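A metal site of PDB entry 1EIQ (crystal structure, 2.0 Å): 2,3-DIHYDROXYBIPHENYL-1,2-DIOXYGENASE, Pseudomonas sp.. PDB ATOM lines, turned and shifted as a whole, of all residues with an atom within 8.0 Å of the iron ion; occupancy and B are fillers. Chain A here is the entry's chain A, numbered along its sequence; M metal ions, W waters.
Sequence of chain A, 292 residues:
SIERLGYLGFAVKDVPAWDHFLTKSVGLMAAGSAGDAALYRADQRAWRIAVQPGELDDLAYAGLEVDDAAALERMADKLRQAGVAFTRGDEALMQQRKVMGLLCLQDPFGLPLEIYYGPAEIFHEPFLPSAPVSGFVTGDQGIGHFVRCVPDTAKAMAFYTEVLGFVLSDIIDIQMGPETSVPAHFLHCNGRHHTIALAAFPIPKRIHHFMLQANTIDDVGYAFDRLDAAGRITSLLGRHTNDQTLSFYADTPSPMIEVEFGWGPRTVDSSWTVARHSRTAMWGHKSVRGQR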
ATOM      1  N   HIS A 145      26.813 -29.011  30.471  1.00  0.00           N
ATOM      2  CA  HIS A 145      25.622 -28.268  30.048  1.00  0.00           C
ATOM      3  C   HIS A 145      24.753 -29.053  29.057  1.00  0.00           C
ATOM      4  O   HIS A 145      25.107 -30.151  28.628  1.00  0.00           O
ATOM      5  CB  HIS A 145      26.019 -26.912  29.429  1.00  0.00           C
ATOM      6  CG  HIS A 145      26.541 -26.996  28.023  1.00  0.00           C
ATOM      7  ND1 HIS A 145      27.831 -26.652  27.695  1.00  0.00           N
ATOM      8  CD2 HIS A 145      25.940 -27.352  26.872  1.00  0.00           C
ATOM      9  CE1 HIS A 145      28.006 -26.798  26.396  1.00  0.00           C
ATOM     10  NE2 HIS A 145      26.875 -27.217  25.862  1.00  0.00           N
ATOM     11  N   PHE A 146      23.589 -28.488  28.747  1.00  0.00           N
ATOM     12  CA  PHE A 146      22.677 -29.098  27.799  1.00  0.00           C
ATOM     13  C   PHE A 146      21.781 -28.048  27.162  1.00  0.00           C
ATOM     14  O   PHE A 146      21.506 -27.002  27.747  1.00  0.00           O
ATOM     15  CB  PHE A 146      21.847 -30.212  28.446  1.00  0.00           C
ATOM     16  CG  PHE A 146      20.783 -29.743  29.422  1.00  0.00           C
ATOM     17  CD1 PHE A 146      19.526 -29.349  28.970  1.00  0.00           C
ATOM     18  CD2 PHE A 146      21.014 -29.795  30.802  1.00  0.00           C
ATOM     19  CE1 PHE A 146      18.508 -29.018  29.871  1.00  0.00           C
ATOM     20  CE2 PHE A 146      20.007 -29.471  31.708  1.00  0.00           C
ATOM     21  CZ  PHE A 146      18.743 -29.083  31.245  1.00  0.00           C
ATOM     22  N   VAL A 147      21.350 -28.345  25.934  1.00  0.00           N
ATOM     23  CA  VAL A 147      20.477 -27.462  25.197  1.00  0.00           C
ATOM     24  C   VAL A 147      19.038 -27.961  25.317  1.00  0.00           C
ATOM     25  O   VAL A 147      18.682 -29.037  24.836  1.00  0.00           O
ATOM     26  CB  VAL A 147      20.859 -27.404  23.701  1.00  0.00           C
ATOM     27  CG1 VAL A 147      19.831 -26.587  22.948  1.00  0.00           C
ATOM     28  CG2 VAL A 147      22.258 -26.813  23.555  1.00  0.00           C
ATOM     29  N   PHE A 186      21.920 -18.601  25.596  1.00  0.00           N
ATOM     30  CA  PHE A 186      22.827 -19.318  26.481  1.00  0.00           C
ATOM     31  C   PHE A 186      22.823 -18.742  27.887  1.00  0.00           C
ATOM     32  O   PHE A 186      23.018 -17.544  28.084  1.00  0.00           O
ATOM     33  CB  PHE A 186      24.237 -19.290  25.862  1.00  0.00           C
ATOM     34  CG  PHE A 186      24.297 -19.948  24.511  1.00  0.00           C
ATOM     35  CD1 PHE A 186      23.857 -19.267  23.379  1.00  0.00           C
ATOM     36  CD2 PHE A 186      24.742 -21.259  24.382  1.00  0.00           C
ATOM     37  CE1 PHE A 186      23.848 -19.893  22.134  1.00  0.00           C
ATOM     38  CE2 PHE A 186      24.734 -21.886  23.138  1.00  0.00           C
ATOM     39  CZ  PHE A 186      24.281 -21.210  22.008  1.00  0.00           C
ATOM     40  N   HIS A 194      27.928 -21.459  29.770  1.00  0.00           N
ATOM     41  CA  HIS A 194      26.523 -21.756  29.863  1.00  0.00           C
ATOM     42  C   HIS A 194      26.305 -23.168  30.381  1.00  0.00           C
ATOM     43  O   HIS A 194      27.067 -24.085  30.078  1.00  0.00           O
ATOM     44  CB  HIS A 194      25.770 -21.499  28.537  1.00  0.00           C
ATOM     45  CG  HIS A 194      26.050 -22.501  27.454  1.00  0.00           C
ATOM     46  ND1 HIS A 194      27.113 -22.385  26.596  1.00  0.00           N
ATOM     47  CD2 HIS A 194      25.359 -23.598  27.066  1.00  0.00           C
ATOM     48  CE1 HIS A 194      27.074 -23.376  25.719  1.00  0.00           C
ATOM     49  NE2 HIS A 194      26.018 -24.125  25.977  1.00  0.00           N
ATOM     50  N   ALA A 197      21.030 -23.876  27.671  1.00  0.00           N
ATOM     51  CA  ALA A 197      20.731 -22.997  26.544  1.00  0.00           C
ATOM     52  C   ALA A 197      19.302 -23.310  26.109  1.00  0.00           C
ATOM     53  O   ALA A 197      18.875 -24.455  26.138  1.00  0.00           O
ATOM     54  CB  ALA A 197      21.705 -23.236  25.391  1.00  0.00           C
ATOM     55  N   HIS A 208      18.497 -31.104  22.873  1.00  0.00           N
ATOM     56  CA  HIS A 208      19.167 -31.363  21.609  1.00  0.00           C
ATOM     57  C   HIS A 208      20.448 -32.175  21.877  1.00  0.00           C
ATOM     58  O   HIS A 208      20.826 -33.043  21.096  1.00  0.00           O
ATOM     59  CB  HIS A 208      19.483 -30.043  20.895  1.00  0.00           C
ATOM     60  CG  HIS A 208      20.457 -30.193  19.757  1.00  0.00           C
ATOM     61  ND1 HIS A 208      21.817 -30.161  19.946  1.00  0.00           N
ATOM     62  CD2 HIS A 208      20.258 -30.416  18.439  1.00  0.00           C
ATOM     63  CE1 HIS A 208      22.424 -30.368  18.782  1.00  0.00           C
ATOM     64  NE2 HIS A 208      21.494 -30.518  17.856  1.00  0.00           N
ATOM     65  N   HIS A 209      21.106 -31.879  23.004  1.00  0.00           N
ATOM     66  CA  HIS A 209      22.322 -32.583  23.387  1.00  0.00           C
ATOM     67  C   HIS A 209      22.801 -32.138  24.763  1.00  0.00           C
ATOM     68  O   HIS A 209      22.337 -31.124  25.298  1.00  0.00           O
ATOM     69  CB  HIS A 209      23.450 -32.317  22.359  1.00  0.00           C
ATOM     70  CG  HIS A 209      24.127 -30.989  22.526  1.00  0.00           C
ATOM     71  ND1 HIS A 209      23.813 -29.880  21.753  1.00  0.00           N
ATOM     72  CD2 HIS A 209      25.082 -30.572  23.393  1.00  0.00           C
ATOM     73  CE1 HIS A 209      24.554 -28.853  22.138  1.00  0.00           C
ATOM     74  NE2 HIS A 209      25.333 -29.246  23.123  1.00  0.00           N
ATOM     75  N   PHE A 210      23.719 -32.919  25.332  1.00  0.00           N
ATOM     76  CA  PHE A 210      24.322 -32.583  26.618  1.00  0.00           C
ATOM     77  C   PHE A 210      25.812 -32.553  26.344  1.00  0.00           C
ATOM     78  O   PHE A 210      26.289 -33.212  25.411  1.00  0.00           O
ATOM     79  CB  PHE A 210      23.952 -33.590  27.722  1.00  0.00           C
ATOM     80  CG  PHE A 210      24.531 -34.975  27.543  1.00  0.00           C
ATOM     81  CD1 PHE A 210      25.654 -35.371  28.262  1.00  0.00           C
ATOM     82  CD2 PHE A 210      23.911 -35.897  26.697  1.00  0.00           C
ATOM     83  CE1 PHE A 210      26.162 -36.674  28.160  1.00  0.00           C
ATOM     84  CE2 PHE A 210      24.404 -37.202  26.589  1.00  0.00           C
ATOM     85  CZ  PHE A 210      25.525 -37.588  27.322  1.00  0.00           C
ATOM     86  N   MET A 211      26.547 -31.796  27.139  1.00  0.00           N
ATOM     87  CA  MET A 211      27.977 -31.655  26.937  1.00  0.00           C
ATOM     88  C   MET A 211      28.830 -31.993  28.145  1.00  0.00           C
ATOM     89  O   MET A 211      28.468 -31.693  29.285  1.00  0.00           O
ATOM     90  CB  MET A 211      28.291 -30.223  26.484  1.00  0.00           C
ATOM     91  CG  MET A 211      29.742 -29.978  26.112  1.00  0.00           C
ATOM     92  SD  MET A 211      30.678 -29.283  27.490  1.00  0.00           S
ATOM     93  CE  MET A 211      32.246 -28.934  26.680  1.00  0.00           C
ATOM     94  N   LEU A 212      29.965 -32.621  27.881  1.00  0.00           N
ATOM     95  CA  LEU A 212      30.934 -32.982  28.916  1.00  0.00           C
ATOM     96  C   LEU A 212      32.257 -32.325  28.498  1.00  0.00           C
ATOM     97  O   LEU A 212      32.604 -32.326  27.309  1.00  0.00           O
ATOM     98  CB  LEU A 212      31.124 -34.509  28.996  1.00  0.00           C
ATOM     99  CG  LEU A 212      30.001 -35.372  29.576  1.00  0.00           C
ATOM    100  CD1 LEU A 212      30.436 -36.833  29.580  1.00  0.00           C
ATOM    101  CD2 LEU A 212      29.672 -34.924  30.989  1.00  0.00           C
ATOM    102  N   HIS A 240      33.257 -23.369  19.016  1.00  0.00           N
ATOM    103  CA  HIS A 240      32.112 -22.465  19.049  1.00  0.00           C
ATOM    104  C   HIS A 240      32.507 -21.003  19.134  1.00  0.00           C
ATOM    105  O   HIS A 240      33.560 -20.645  19.662  1.00  0.00           O
ATOM    106  CB  HIS A 240      31.198 -22.838  20.221  1.00  0.00           C
ATOM    107  CG  HIS A 240      30.421 -24.096  19.996  1.00  0.00           C
ATOM    108  ND1 HIS A 240      29.437 -24.202  19.033  1.00  0.00           N
ATOM    109  CD2 HIS A 240      30.487 -25.303  20.597  1.00  0.00           C
ATOM    110  CE1 HIS A 240      28.937 -25.420  19.052  1.00  0.00           C
ATOM    111  NE2 HIS A 240      29.559 -26.110  19.986  1.00  0.00           N
ATOM    112  N   ASN A 242      30.643 -18.421  20.679  1.00  0.00           N
ATOM    113  CA  ASN A 242      30.395 -17.818  21.982  1.00  0.00           C
ATOM    114  C   ASN A 242      31.217 -18.342  23.176  1.00  0.00           C
ATOM    115  O   ASN A 242      31.847 -17.548  23.851  1.00  0.00           O
ATOM    116  CB  ASN A 242      28.887 -17.856  22.302  1.00  0.00           C
ATOM    117  CG  ASN A 242      28.307 -19.262  22.333  1.00  0.00           C
ATOM    118  OD1 ASN A 242      28.873 -20.217  21.806  1.00  0.00           O
ATOM    119  ND2 ASN A 242      27.145 -19.386  22.969  1.00  0.00           N
ATOM    120  N   ASP A 243      31.207 -19.655  23.443  1.00  0.00           N
ATOM    121  CA  ASP A 243      31.962 -20.171  24.584  1.00  0.00           C
ATOM    122  C   ASP A 243      33.380 -20.637  24.229  1.00  0.00           C
ATOM    123  O   ASP A 243      34.175 -20.922  25.112  1.00  0.00           O
ATOM    124  CB  ASP A 243      31.206 -21.308  25.288  1.00  0.00           C
ATOM    125  CG  ASP A 243      31.094 -22.573  24.451  1.00  0.00           C
ATOM    126  OD1 ASP A 243      30.584 -23.596  24.974  1.00  0.00           O
ATOM    127  OD2 ASP A 243      31.510 -22.566  23.276  1.00  0.00           O
ATOM    128  N   THR A 245      34.242 -23.385  22.946  1.00  0.00           N
ATOM    129  CA  THR A 245      34.441 -24.788  23.243  1.00  0.00           C
ATOM    130  C   THR A 245      34.917 -25.455  21.961  1.00  0.00           C
ATOM    131  O   THR A 245      34.307 -25.264  20.898  1.00  0.00           O
ATOM    132  CB  THR A 245      33.132 -25.491  23.688  1.00  0.00           C
ATOM    133  OG1 THR A 245      32.801 -25.098  25.019  1.00  0.00           O
ATOM    134  CG2 THR A 245      33.291 -27.009  23.660  1.00  0.00           C
ATOM    135  N   SER A 247      35.162 -28.785  20.138  1.00  0.00           N
ATOM    136  CA  SER A 247      34.505 -30.066  20.293  1.00  0.00           C
ATOM    137  C   SER A 247      33.996 -30.712  19.008  1.00  0.00           C
ATOM    138  O   SER A 247      34.176 -30.187  17.916  1.00  0.00           O
ATOM    139  CB  SER A 247      33.312 -29.887  21.223  1.00  0.00           C
ATOM    140  OG  SER A 247      32.369 -28.990  20.640  1.00  0.00           O
ATOM    141  N   TYR A 249      30.490 -33.490  17.839  1.00  0.00           N
ATOM    142  CA  TYR A 249      29.215 -34.031  18.299  1.00  0.00           C
ATOM    143  C   TYR A 249      29.044 -35.465  17.830  1.00  0.00           C
ATOM    144  O   TYR A 249      29.672 -35.892  16.866  1.00  0.00           O
ATOM    145  CB  TYR A 249      28.057 -33.188  17.765  1.00  0.00           C
ATOM    146  CG  TYR A 249      27.962 -31.818  18.370  1.00  0.00           C
ATOM    147  CD1 TYR A 249      27.000 -31.524  19.330  1.00  0.00           C
ATOM    148  CD2 TYR A 249      28.817 -30.796  17.961  1.00  0.00           C
ATOM    149  CE1 TYR A 249      26.882 -30.247  19.871  1.00  0.00           C
ATOM    150  CE2 TYR A 249      28.710 -29.511  18.490  1.00  0.00           C
ATOM    151  CZ  TYR A 249      27.745 -29.250  19.452  1.00  0.00           C
ATOM    152  OH  TYR A 249      27.613 -27.985  19.972  1.00  0.00           O
ATOM    153  N   VAL A 259      25.540 -35.959  21.877  1.00  0.00           N
ATOM    154  CA  VAL A 259      26.468 -35.670  22.953  1.00  0.00           C
ATOM    155  C   VAL A 259      27.556 -34.787  22.356  1.00  0.00           C
ATOM    156  O   VAL A 259      27.918 -34.922  21.178  1.00  0.00           O
ATOM    157  CB  VAL A 259      27.095 -36.949  23.538  1.00  0.00           C
ATOM    158  CG1 VAL A 259      27.972 -37.641  22.498  1.00  0.00           C
ATOM    159  CG2 VAL A 259      27.905 -36.598  24.766  1.00  0.00           C
ATOM    160  N   GLU A 260      28.067 -33.859  23.160  1.00  0.00           N
ATOM    161  CA  GLU A 260      29.143 -32.991  22.715  1.00  0.00           C
ATOM    162  C   GLU A 260      30.298 -33.235  23.675  1.00  0.00           C
ATOM    163  O   GLU A 260      30.130 -33.206  24.894  1.00  0.00           O
ATOM    164  CB  GLU A 260      28.715 -31.529  22.753  1.00  0.00           C
ATOM    165  CG  GLU A 260      29.836 -30.581  22.382  1.00  0.00           C
ATOM    166  CD  GLU A 260      29.469 -29.134  22.549  1.00  0.00           C
ATOM    167  OE1 GLU A 260      28.486 -28.850  23.252  1.00  0.00           O
ATOM    168  OE2 GLU A 260      30.176 -28.271  21.963  1.00  0.00           O
ATOM    169  N   PHE A 261      31.472 -33.489  23.108  1.00  0.00           N
ATOM    170  CA  PHE A 261      32.679 -33.755  23.884  1.00  0.00           C
ATOM    171  C   PHE A 261      33.669 -32.640  23.526  1.00  0.00           C
ATOM    172  O   PHE A 261      34.172 -32.594  22.402  1.00  0.00           O
ATOM    173  CB  PHE A 261      33.221 -35.135  23.478  1.00  0.00           C
ATOM    174  CG  PHE A 261      34.192 -35.737  24.443  1.00  0.00           C
ATOM    175  CD1 PHE A 261      33.779 -36.706  25.354  1.00  0.00           C
ATOM    176  CD2 PHE A 261      35.540 -35.384  24.404  1.00  0.00           C
ATOM    177  CE1 PHE A 261      34.700 -37.335  26.206  1.00  0.00           C
ATOM    178  CE2 PHE A 261      36.467 -35.992  25.249  1.00  0.00           C
ATOM    179  CZ  PHE A 261      36.050 -36.970  26.159  1.00  0.00           C
ATOM    180  N   HIS A 285      33.282 -27.948  12.921  1.00  0.00           N
ATOM    181  CA  HIS A 285      31.918 -28.366  13.238  1.00  0.00           C
ATOM    182  C   HIS A 285      31.111 -28.737  11.982  1.00  0.00           C
ATOM    183  O   HIS A 285      29.875 -28.762  12.019  1.00  0.00           O
ATOM    184  CB  HIS A 285      31.182 -27.266  14.010  1.00  0.00           C
ATOM    185  CG  HIS A 285      31.470 -27.259  15.487  1.00  0.00           C
ATOM    186  ND1 HIS A 285      31.928 -28.372  16.161  1.00  0.00           N
ATOM    187  CD2 HIS A 285      31.385 -26.266  16.401  1.00  0.00           C
ATOM    188  CE1 HIS A 285      32.102 -28.063  17.437  1.00  0.00           C
ATOM    189  NE2 HIS A 285      31.783 -26.800  17.611  1.00  0.00           N
HETATM  190 FE    FE M   1      26.933 -27.411  23.554  1.00  0.00          FE
HETATM  191  O   HOH W   1      28.918 -25.591  23.334  1.00  0.00           O
HETATM  192  O   HOH W   2      25.718 -25.522  23.454  1.00  0.00           O
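Tyr 249 touches the iron ion (OH to FE, 3.7 Å).
The nearest printed residue that does not touch the iron ion is His 194 (4.2 Å).
The iron ion is bound by the side-chain carboxylate of Glu 260 (2.1 Å), water W2 (2.2 Å), a ring nitrogen (NE2) of His 145 (2.3 Å) and a ring nitrogen (NE2) of His 209 (2.5 Å).
Slightly farther from the iron ion lies water W1 (2.7 Å).
N of Met 211 lies within hydrogen-bond range of O of His 145 (2.6 Å).
The side-chain carboxylate of Glu 260 lies within hydrogen-bond range of the side-chain hydroxyl of Ser 247 (2.7 Å).
A ring nitrogen (NE2) of His 145 sits close to a ring nitrogen (NE2) of His 194 (3.2 Å).
N of Glu 260 is in hydrogen-bond range of O of Phe 210, at 2.9 Å.
OE2 of Glu 260 sits at hydrogen-bond distance from OH of Tyr 249 (3.3 Å).
The side-chain hydroxyl (OH) of Tyr 249 sits at hydrogen-bond distance from a ring nitrogen (NE2) of His 240 (2.7 Å).
O of Glu 260 lies within hydrogen-bond range of N of Leu 212 (3.0 Å).
A ring nitrogen (ND1) of His 209 sits at hydrogen-bond distance from a ring nitrogen (ND1) of His 208.
Water W1 lies within hydrogen-bond range of the side-chain carboxylate of Asp 243 (3.1 Å), the side-chain carboxylate of Glu 260 (3.3 Å) and a ring nitrogen (NE2) of His 240 (3.4 Å).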
